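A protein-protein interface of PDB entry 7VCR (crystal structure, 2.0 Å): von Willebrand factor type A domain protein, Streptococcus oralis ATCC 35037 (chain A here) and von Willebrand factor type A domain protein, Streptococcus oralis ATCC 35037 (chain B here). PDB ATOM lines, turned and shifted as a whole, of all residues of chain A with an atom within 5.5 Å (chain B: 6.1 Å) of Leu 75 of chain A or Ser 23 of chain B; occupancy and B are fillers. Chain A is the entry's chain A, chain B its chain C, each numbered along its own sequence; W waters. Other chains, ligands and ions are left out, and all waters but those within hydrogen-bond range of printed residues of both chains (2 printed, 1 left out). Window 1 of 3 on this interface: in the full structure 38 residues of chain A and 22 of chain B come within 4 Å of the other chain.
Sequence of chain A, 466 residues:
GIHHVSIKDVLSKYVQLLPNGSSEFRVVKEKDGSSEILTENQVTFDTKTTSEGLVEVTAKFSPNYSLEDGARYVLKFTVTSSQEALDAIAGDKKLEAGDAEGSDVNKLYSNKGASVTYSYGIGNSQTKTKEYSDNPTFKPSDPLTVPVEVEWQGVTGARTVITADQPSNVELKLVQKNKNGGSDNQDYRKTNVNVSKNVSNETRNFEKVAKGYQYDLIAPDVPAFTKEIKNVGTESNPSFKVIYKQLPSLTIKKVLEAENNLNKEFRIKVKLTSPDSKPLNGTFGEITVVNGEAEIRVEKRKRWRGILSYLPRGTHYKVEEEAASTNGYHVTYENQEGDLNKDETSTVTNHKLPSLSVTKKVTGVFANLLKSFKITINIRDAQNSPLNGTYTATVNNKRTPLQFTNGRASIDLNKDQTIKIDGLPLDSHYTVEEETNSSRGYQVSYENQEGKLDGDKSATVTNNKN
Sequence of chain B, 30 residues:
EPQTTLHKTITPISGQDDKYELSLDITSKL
NH2 of Arg 26 of chain A lies within salt-bridge range of OE2 of Glu 21 of chain B, 2.9 Å away.
The backbone NH of Leu 22 of chain B lies within hydrogen-bond range of the backbone carbonyl oxygen of Phe 77 of chain A, at 2.8 Å.
OG of Ser 23 of chain B lies within hydrogen-bond range of NZ of Lys 76 of chain A (3.4 Å).
The backbone NH (N) of Leu 75 of chain A sits at hydrogen-bond distance from the backbone carbonyl oxygen (O) of Leu 24 of chain B, at 2.8 Å.
The guanidinium group of Arg 72 of chain A is in salt-bridge range of the side-chain carboxylate of Asp 25 of chain B (2.8 Å).
The side-chain carboxylate (OD1) of Asp 25 of chain B lies within hydrogen-bond range of the backbone NH (N) of His 7 of chain B (2.7 Å).
The backbone NH of Ser 23 of chain B sits at hydrogen-bond distance from the backbone carbonyl oxygen of Thr 9 of chain B.
O of Ile 7 of chain A lies within hydrogen-bond range of N of Ala 59 of chain A (2.7 Å).
O of Arg 26 of chain A lies within hydrogen-bond range of N of Lys 76 of chain A.
The backbone NH (N) of Val 28 of chain A is in hydrogen-bond range of the backbone carbonyl oxygen (O) of Val 74 of chain A, at 2.8 Å.
Among the printed residues, merely in contact across the chains: Ile 7 of chain A with Leu 24 of chain B (3.8 Å), Lys 8 of chain A with Leu 24 of chain B (3.8 Å), Arg 72 of chain A with Ser 23 of chain B (3.9 Å), Tyr 73 of chain A with Asp 25 of chain B (3.2 Å), Val 74 of chain A with Ser 23 of chain B (3.2 Å), Val 74 of chain A with Leu 24 of chain B (3.5 Å), Val 74 of chain A with Asp 25 of chain B (3.8 Å), Leu 75 of chain A with Leu 22 of chain B (3.6 Å), Leu 75 of chain A with Ser 23 of chain B (3.4 Å), Lys 76 of chain A with Leu 22 of chain B (3.3 Å) and Phe 77 of chain A with Glu 21 of chain B (3.5 Å).
Ala 59 of chain A touches none of the printed residues of chain B.
Printed residues of chain B within 4 Å of Tyr 73 of chain A: Asp 25.
Of the printed residues of chain B, Val 74 of chain A touches Ser 23, Leu 24 and Asp 25.
Leu 75 of chain A touches just these residues of chain B: Leu 22, Ser 23 and Leu 24.
Ser 23 of chain B touches four residues of chain A.
The nearest residue of chain B that does not touch Leu 75 of chain A is Asp 25 of chain B (4.8 Å).
The nearest residue of chain A that does not touch Ser 23 of chain B is Phe 77 of chain A (5.4 Å).
Of the 15 printed residues of chain A, 9 touch a printed residue of chain B.
Printed residues of chain A that touch a printed residue of chain B: Ile 7, Lys 8, Arg 26, Arg 72, Tyr 73, Val 74, Leu 75, Lys 76 and Phe 77.
Printed residues of chain B that touch a printed residue of chain A: Glu 21, Leu 22, Ser 23, Leu 24 and Asp 25.
Among the printed residues, 16 pairs touch across the chains.
Among the printed residues, Asp or Glu carboxylates within 4 Å of a Lys or Arg side-chain nitrogen of the other chain: Arg 26 of chain A with Glu 21 of chain B and Arg 72 of chain A with Asp 25 of chain B.
Water W2 lies within hydrogen-bond range of the side-chain hydroxyl (OG) of Ser 23 of chain B (2.5 Å), the backbone carbonyl oxygen (O) of His 7 of chain B (3.1 Å), the guanidinium group (NH2) of Arg 72 of chain A (3.2 Å) and the side-chain carboxylate (OD2) of Asp 25 of chain B (3.3 Å).
Water W1 lies within hydrogen-bond range of the side-chain carboxylate of Glu 21 of chain B and the guanidinium group of Arg 26 of chain A.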
ATOM      1  N   ILE A   7       3.810 -21.757   2.340  1.00  0.00           N
ATOM      2  CA  ILE A   7       3.868 -21.931   3.769  1.00  0.00           C
ATOM      3  C   ILE A   7       2.767 -21.071   4.377  1.00  0.00           C
ATOM      4  O   ILE A   7       2.631 -19.877   4.032  1.00  0.00           O
ATOM      5  CB  ILE A   7       5.254 -21.480   4.246  1.00  0.00           C
ATOM      6  CG1 ILE A   7       6.385 -22.325   3.657  1.00  0.00           C
ATOM      7  CG2 ILE A   7       5.372 -21.422   5.781  1.00  0.00           C
ATOM      8  CD1 ILE A   7       7.742 -21.590   3.796  1.00  0.00           C
ATOM      9  N   LYS A   8       2.080 -21.612   5.383  1.00  0.00           N
ATOM     10  CA  LYS A   8       0.865 -20.974   5.893  1.00  0.00           C
ATOM     11  C   LYS A   8       0.976 -20.961   7.418  1.00  0.00           C
ATOM     12  O   LYS A   8       1.409 -21.948   8.014  1.00  0.00           O
ATOM     13  CB  LYS A   8      -0.312 -21.855   5.444  1.00  0.00           C
ATOM     14  CG  LYS A   8      -1.692 -21.525   5.971  1.00  0.00           C
ATOM     15  CD  LYS A   8      -2.596 -22.778   6.286  1.00  0.00           C
ATOM     16  CE  LYS A   8      -2.233 -23.327   7.666  1.00  0.00           C
ATOM     17  NZ  LYS A   8      -2.916 -24.564   8.128  1.00  0.00           N
ATOM     18  N   PHE A  25       7.315  -9.235   5.811  1.00  0.00           N
ATOM     19  CA  PHE A  25       7.306 -10.617   5.374  1.00  0.00           C
ATOM     20  C   PHE A  25       8.519 -10.850   4.464  1.00  0.00           C
ATOM     21  O   PHE A  25       8.786 -10.103   3.538  1.00  0.00           O
ATOM     22  CB  PHE A  25       5.983 -10.967   4.684  1.00  0.00           C
ATOM     23  CG  PHE A  25       4.752 -10.898   5.524  1.00  0.00           C
ATOM     24  CD1 PHE A  25       4.406 -11.917   6.385  1.00  0.00           C
ATOM     25  CD2 PHE A  25       3.900  -9.813   5.410  1.00  0.00           C
ATOM     26  CE1 PHE A  25       3.279 -11.785   7.211  1.00  0.00           C
ATOM     27  CE2 PHE A  25       2.770  -9.720   6.209  1.00  0.00           C
ATOM     28  CZ  PHE A  25       2.468 -10.712   7.111  1.00  0.00           C
ATOM     29  N   ARG A  26       9.256 -11.946   4.730  1.00  0.00           N
ATOM     30  CA  ARG A  26      10.341 -12.324   3.843  1.00  0.00           C
ATOM     31  C   ARG A  26      10.581 -13.842   3.915  1.00  0.00           C
ATOM     32  O   ARG A  26      10.245 -14.457   4.909  1.00  0.00           O
ATOM     33  CB  ARG A  26      11.641 -11.572   4.179  1.00  0.00           C
ATOM     34  CG  ARG A  26      12.235 -11.914   5.543  1.00  0.00           C
ATOM     35  CD  ARG A  26      13.044 -10.693   6.033  1.00  0.00           C
ATOM     36  NE  ARG A  26      13.635 -11.038   7.336  1.00  0.00           N
ATOM     37  CZ  ARG A  26      13.002 -10.847   8.524  1.00  0.00           C
ATOM     38  NH1 ARG A  26      11.758 -10.347   8.592  1.00  0.00           N
ATOM     39  NH2 ARG A  26      13.622 -11.172   9.631  1.00  0.00           N
ATOM     40  N   VAL A  27      11.100 -14.436   2.824  1.00  0.00           N
ATOM     41  CA  VAL A  27      11.571 -15.811   2.863  1.00  0.00           C
ATOM     42  C   VAL A  27      13.086 -15.768   2.617  1.00  0.00           C
ATOM     43  O   VAL A  27      13.515 -15.160   1.630  1.00  0.00           O
ATOM     44  CB  VAL A  27      10.834 -16.701   1.823  1.00  0.00           C
ATOM     45  CG1 VAL A  27      11.502 -18.114   1.731  1.00  0.00           C
ATOM     46  CG2 VAL A  27       9.345 -16.812   2.160  1.00  0.00           C
ATOM     47  N   VAL A  28      13.859 -16.331   3.556  1.00  0.00           N
ATOM     48  CA  VAL A  28      15.309 -16.363   3.427  1.00  0.00           C
ATOM     49  C   VAL A  28      15.680 -17.790   2.991  1.00  0.00           C
ATOM     50  O   VAL A  28      15.167 -18.780   3.548  1.00  0.00           O
ATOM     51  CB  VAL A  28      16.023 -16.014   4.761  1.00  0.00           C
ATOM     52  CG1 VAL A  28      17.535 -16.156   4.645  1.00  0.00           C
ATOM     53  CG2 VAL A  28      15.684 -14.575   5.181  1.00  0.00           C
ATOM     54  N   PHE A  45       3.189 -12.864  -0.787  1.00  0.00           N
ATOM     55  CA  PHE A  45       2.589 -13.030   0.554  1.00  0.00           C
ATOM     56  C   PHE A  45       1.127 -12.639   0.486  1.00  0.00           C
ATOM     57  O   PHE A  45       0.764 -11.637  -0.159  1.00  0.00           O
ATOM     58  CB  PHE A  45       3.331 -12.112   1.524  1.00  0.00           C
ATOM     59  CG  PHE A  45       4.797 -12.433   1.531  1.00  0.00           C
ATOM     60  CD1 PHE A  45       5.262 -13.561   2.177  1.00  0.00           C
ATOM     61  CD2 PHE A  45       5.702 -11.626   0.852  1.00  0.00           C
ATOM     62  CE1 PHE A  45       6.597 -13.894   2.175  1.00  0.00           C
ATOM     63  CE2 PHE A  45       7.051 -11.959   0.872  1.00  0.00           C
ATOM     64  CZ  PHE A  45       7.478 -13.108   1.520  1.00  0.00           C
ATOM     65  N   VAL A  57      -1.662 -16.150   7.298  1.00  0.00           N
ATOM     66  CA  VAL A  57      -0.593 -15.541   6.520  1.00  0.00           C
ATOM     67  C   VAL A  57      -0.090 -16.656   5.574  1.00  0.00           C
ATOM     68  O   VAL A  57       0.129 -17.769   6.034  1.00  0.00           O
ATOM     69  CB  VAL A  57       0.495 -15.105   7.522  1.00  0.00           C
ATOM     70  CG1 VAL A  57       1.809 -14.846   6.857  1.00  0.00           C
ATOM     71  CG2 VAL A  57       0.058 -13.817   8.262  1.00  0.00           C
ATOM     72  N   ALA A  59       2.854 -17.582   2.546  1.00  0.00           N
ATOM     73  CA  ALA A  59       3.909 -17.251   1.596  1.00  0.00           C
ATOM     74  C   ALA A  59       3.773 -18.227   0.422  1.00  0.00           C
ATOM     75  O   ALA A  59       4.036 -19.436   0.630  1.00  0.00           O
ATOM     76  CB  ALA A  59       5.266 -17.505   2.179  1.00  0.00           C
ATOM     77  N   ARG A  72      17.826 -24.504   3.514  1.00  0.00           N
ATOM     78  CA  ARG A  72      16.706 -24.129   4.369  1.00  0.00           C
ATOM     79  C   ARG A  72      15.994 -22.886   3.832  1.00  0.00           C
ATOM     80  O   ARG A  72      16.599 -21.847   3.599  1.00  0.00           O
ATOM     81  CB  ARG A  72      17.261 -23.964   5.777  1.00  0.00           C
ATOM     82  CG  ARG A  72      16.234 -23.721   6.871  1.00  0.00           C
ATOM     83  CD  ARG A  72      17.036 -23.129   8.055  1.00  0.00           C
ATOM     84  NE  ARG A  72      16.096 -22.815   9.090  1.00  0.00           N
ATOM     85  CZ  ARG A  72      16.108 -21.714   9.848  1.00  0.00           C
ATOM     86  NH1 ARG A  72      17.042 -20.790   9.682  1.00  0.00           N
ATOM     87  NH2 ARG A  72      15.193 -21.578  10.793  1.00  0.00           N
ATOM     88  N   TYR A  73      14.680 -22.982   3.681  1.00  0.00           N
ATOM     89  CA  TYR A  73      13.854 -21.802   3.323  1.00  0.00           C
ATOM     90  C   TYR A  73      12.999 -21.445   4.532  1.00  0.00           C
ATOM     91  O   TYR A  73      12.440 -22.348   5.130  1.00  0.00           O
ATOM     92  CB  TYR A  73      12.900 -22.125   2.171  1.00  0.00           C
ATOM     93  CG  TYR A  73      13.640 -22.324   0.871  1.00  0.00           C
ATOM     94  CD1 TYR A  73      14.258 -23.549   0.569  1.00  0.00           C
ATOM     95  CD2 TYR A  73      13.826 -21.277  -0.005  1.00  0.00           C
ATOM     96  CE1 TYR A  73      14.911 -23.722  -0.630  1.00  0.00           C
ATOM     97  CE2 TYR A  73      14.456 -21.456  -1.238  1.00  0.00           C
ATOM     98  CZ  TYR A  73      15.041 -22.683  -1.523  1.00  0.00           C
ATOM     99  OH  TYR A  73      15.739 -22.927  -2.702  1.00  0.00           O
ATOM    100  N   VAL A  74      13.072 -20.196   4.985  1.00  0.00           N
ATOM    101  CA  VAL A  74      12.419 -19.820   6.241  1.00  0.00           C
ATOM    102  C   VAL A  74      11.616 -18.519   6.024  1.00  0.00           C
ATOM    103  O   VAL A  74      12.141 -17.502   5.496  1.00  0.00           O
ATOM    104  CB  VAL A  74      13.458 -19.694   7.353  1.00  0.00           C
ATOM    105  CG1 VAL A  74      14.479 -18.687   6.971  1.00  0.00           C
ATOM    106  CG2 VAL A  74      12.855 -19.260   8.688  1.00  0.00           C
ATOM    107  N   LEU A  75      10.306 -18.643   6.265  1.00  0.00           N
ATOM    108  CA  LEU A  75       9.415 -17.498   6.258  1.00  0.00           C
ATOM    109  C   LEU A  75       9.627 -16.754   7.582  1.00  0.00           C
ATOM    110  O   LEU A  75       9.532 -17.400   8.639  1.00  0.00           O
ATOM    111  CB  LEU A  75       7.984 -18.045   6.213  1.00  0.00           C
ATOM    112  CG  LEU A  75       6.911 -16.982   6.509  1.00  0.00           C
ATOM    113  CD1 LEU A  75       6.949 -15.833   5.471  1.00  0.00           C
ATOM    114  CD2 LEU A  75       5.566 -17.661   6.524  1.00  0.00           C
ATOM    115  N   LYS A  76       9.959 -15.444   7.529  1.00  0.00           N
ATOM    116  CA  LYS A  76      10.100 -14.676   8.786  1.00  0.00           C
ATOM    117  C   LYS A  76       9.125 -13.492   8.737  1.00  0.00           C
ATOM    118  O   LYS A  76       8.952 -12.884   7.667  1.00  0.00           O
ATOM    119  CB  LYS A  76      11.564 -14.185   8.883  1.00  0.00           C
ATOM    120  CG  LYS A  76      12.481 -15.357   9.253  1.00  0.00           C
ATOM    121  CD  LYS A  76      13.924 -14.962   9.391  1.00  0.00           C
ATOM    122  CE  LYS A  76      14.844 -16.063   9.916  1.00  0.00           C
ATOM    123  NZ  LYS A  76      14.316 -16.835  11.085  1.00  0.00           N
ATOM    124  N   PHE A  77       8.476 -13.189   9.870  1.00  0.00           N
ATOM    125  CA  PHE A  77       7.688 -11.963   9.997  1.00  0.00           C
ATOM    126  C   PHE A  77       7.510 -11.646  11.478  1.00  0.00           C
ATOM    127  O   PHE A  77       7.678 -12.519  12.358  1.00  0.00           O
ATOM    128  CB  PHE A  77       6.313 -12.034   9.298  1.00  0.00           C
ATOM    129  CG  PHE A  77       5.421 -13.174   9.750  1.00  0.00           C
ATOM    130  CD1 PHE A  77       5.595 -14.474   9.287  1.00  0.00           C
ATOM    131  CD2 PHE A  77       4.404 -12.962  10.675  1.00  0.00           C
ATOM    132  CE1 PHE A  77       4.738 -15.501   9.660  1.00  0.00           C
ATOM    133  CE2 PHE A  77       3.529 -13.976  11.047  1.00  0.00           C
ATOM    134  CZ  PHE A  77       3.716 -15.284  10.556  1.00  0.00           C
ATOM    135  N   HIS B   7      10.405 -26.725  10.765  1.00  0.00           N
ATOM    136  CA  HIS B   7      10.545 -26.249  12.140  1.00  0.00           C
ATOM    137  C   HIS B   7       9.880 -24.857  12.226  1.00  0.00           C
ATOM    138  O   HIS B   7      10.052 -24.024  11.318  1.00  0.00           O
ATOM    139  CB  HIS B   7      12.000 -26.082  12.560  1.00  0.00           C
ATOM    140  CG  HIS B   7      12.789 -27.349  12.464  1.00  0.00           C
ATOM    141  ND1 HIS B   7      12.796 -28.318  13.468  1.00  0.00           N
ATOM    142  CD2 HIS B   7      13.580 -27.833  11.471  1.00  0.00           C
ATOM    143  CE1 HIS B   7      13.541 -29.350  13.093  1.00  0.00           C
ATOM    144  NE2 HIS B   7      14.034 -29.068  11.875  1.00  0.00           N
ATOM    145  N   LYS B   8       9.183 -24.610  13.336  1.00  0.00           N
ATOM    146  CA  LYS B   8       8.563 -23.329  13.596  1.00  0.00           C
ATOM    147  C   LYS B   8       8.947 -22.849  15.000  1.00  0.00           C
ATOM    148  O   LYS B   8       8.752 -23.597  15.992  1.00  0.00           O
ATOM    149  CB  LYS B   8       7.028 -23.408  13.517  1.00  0.00           C
ATOM    150  CG  LYS B   8       6.304 -22.087  13.882  1.00  0.00           C
ATOM    151  CD  LYS B   8       4.823 -22.475  13.943  1.00  0.00           C
ATOM    152  CE  LYS B   8       3.957 -21.257  14.142  1.00  0.00           C
ATOM    153  NZ  LYS B   8       2.625 -21.665  14.647  1.00  0.00           N
ATOM    154  N   THR B   9       9.445 -21.585  15.069  1.00  0.00           N
ATOM    155  CA  THR B   9       9.739 -20.978  16.382  1.00  0.00           C
ATOM    156  C   THR B   9       9.138 -19.572  16.469  1.00  0.00           C
ATOM    157  O   THR B   9       8.872 -18.920  15.438  1.00  0.00           O
ATOM    158  CB  THR B   9      11.264 -20.881  16.652  1.00  0.00           C
ATOM    159  OG1 THR B   9      11.757 -20.142  15.527  1.00  0.00           O
ATOM    160  CG2 THR B   9      12.022 -22.224  16.598  1.00  0.00           C
ATOM    161  N   ILE B  10       9.006 -19.059  17.703  1.00  0.00           N
ATOM    162  CA  ILE B  10       8.749 -17.633  17.922  1.00  0.00           C
ATOM    163  C   ILE B  10       9.818 -17.113  18.883  1.00  0.00           C
ATOM    164  O   ILE B  10      10.230 -17.821  19.771  1.00  0.00           O
ATOM    165  CB  ILE B  10       7.321 -17.426  18.430  1.00  0.00           C
ATOM    166  CG1 ILE B  10       6.903 -15.961  18.278  1.00  0.00           C
ATOM    167  CG2 ILE B  10       7.197 -17.945  19.869  1.00  0.00           C
ATOM    168  CD1 ILE B  10       5.471 -15.579  18.686  1.00  0.00           C
ATOM    169  N   GLU B  21       9.340 -12.447  16.647  1.00  0.00           N
ATOM    170  CA  GLU B  21       9.558 -12.830  15.257  1.00  0.00           C
ATOM    171  C   GLU B  21       9.151 -14.297  15.111  1.00  0.00           C
ATOM    172  O   GLU B  21       9.612 -15.156  15.885  1.00  0.00           O
ATOM    173  CB  GLU B  21      11.045 -12.667  14.910  1.00  0.00           C
ATOM    174  CG  GLU B  21      11.243 -13.159  13.477  1.00  0.00           C
ATOM    175  CD  GLU B  21      12.567 -12.670  12.940  1.00  0.00           C
ATOM    176  OE1 GLU B  21      13.554 -13.407  13.215  1.00  0.00           O
ATOM    177  OE2 GLU B  21      12.623 -11.558  12.292  1.00  0.00           O
ATOM    178  N   LEU B  22       8.237 -14.566  14.203  1.00  0.00           N
ATOM    179  CA  LEU B  22       7.876 -15.953  13.887  1.00  0.00           C
ATOM    180  C   LEU B  22       8.796 -16.423  12.760  1.00  0.00           C
ATOM    181  O   LEU B  22       9.105 -15.645  11.810  1.00  0.00           O
ATOM    182  CB  LEU B  22       6.411 -16.044  13.392  1.00  0.00           C
ATOM    183  CG  LEU B  22       5.438 -16.175  14.581  1.00  0.00           C
ATOM    184  CD1 LEU B  22       3.979 -15.834  14.193  1.00  0.00           C
ATOM    185  CD2 LEU B  22       5.500 -17.635  15.051  1.00  0.00           C
ATOM    186  N   SER B  23       9.155 -17.730  12.838  1.00  0.00           N
ATOM    187  CA  SER B  23      10.011 -18.342  11.837  1.00  0.00           C
ATOM    188  C   SER B  23       9.423 -19.698  11.452  1.00  0.00           C
ATOM    189  O   SER B  23       9.215 -20.583  12.316  1.00  0.00           O
ATOM    190  CB  SER B  23      11.349 -18.461  12.496  1.00  0.00           C
ATOM    191  OG  SER B  23      12.116 -19.389  11.780  1.00  0.00           O
ATOM    192  N   LEU B  24       9.032 -19.837  10.174  1.00  0.00           N
ATOM    193  CA  LEU B  24       8.440 -21.115   9.723  1.00  0.00           C
ATOM    194  C   LEU B  24       9.316 -21.647   8.578  1.00  0.00           C
ATOM    195  O   LEU B  24       9.436 -20.971   7.550  1.00  0.00           O
ATOM    196  CB  LEU B  24       7.010 -20.906   9.196  1.00  0.00           C
ATOM    197  CG  LEU B  24       5.994 -20.776  10.341  1.00  0.00           C
ATOM    198  CD1 LEU B  24       5.919 -19.340  10.796  1.00  0.00           C
ATOM    199  CD2 LEU B  24       4.617 -21.262   9.931  1.00  0.00           C
ATOM    200  N   ASP B  25      10.020 -22.779   8.832  1.00  0.00           N
ATOM    201  CA  ASP B  25      10.966 -23.189   7.805  1.00  0.00           C
ATOM    202  C   ASP B  25      10.600 -24.529   7.154  1.00  0.00           C
ATOM    203  O   ASP B  25       9.667 -25.240   7.590  1.00  0.00           O
ATOM    204  CB  ASP B  25      12.383 -23.172   8.309  1.00  0.00           C
ATOM    205  CG  ASP B  25      12.829 -24.336   9.190  1.00  0.00           C
ATOM    206  OD1 ASP B  25      12.197 -25.472   9.169  1.00  0.00           O
ATOM    207  OD2 ASP B  25      13.761 -24.061   9.963  1.00  0.00           O
HETATM  208  O   HOH W   1      10.755 -10.067  11.316  1.00  0.00           O
HETATM  209  O   HOH W   2      12.182 -21.862  11.847  1.00  0.00           O
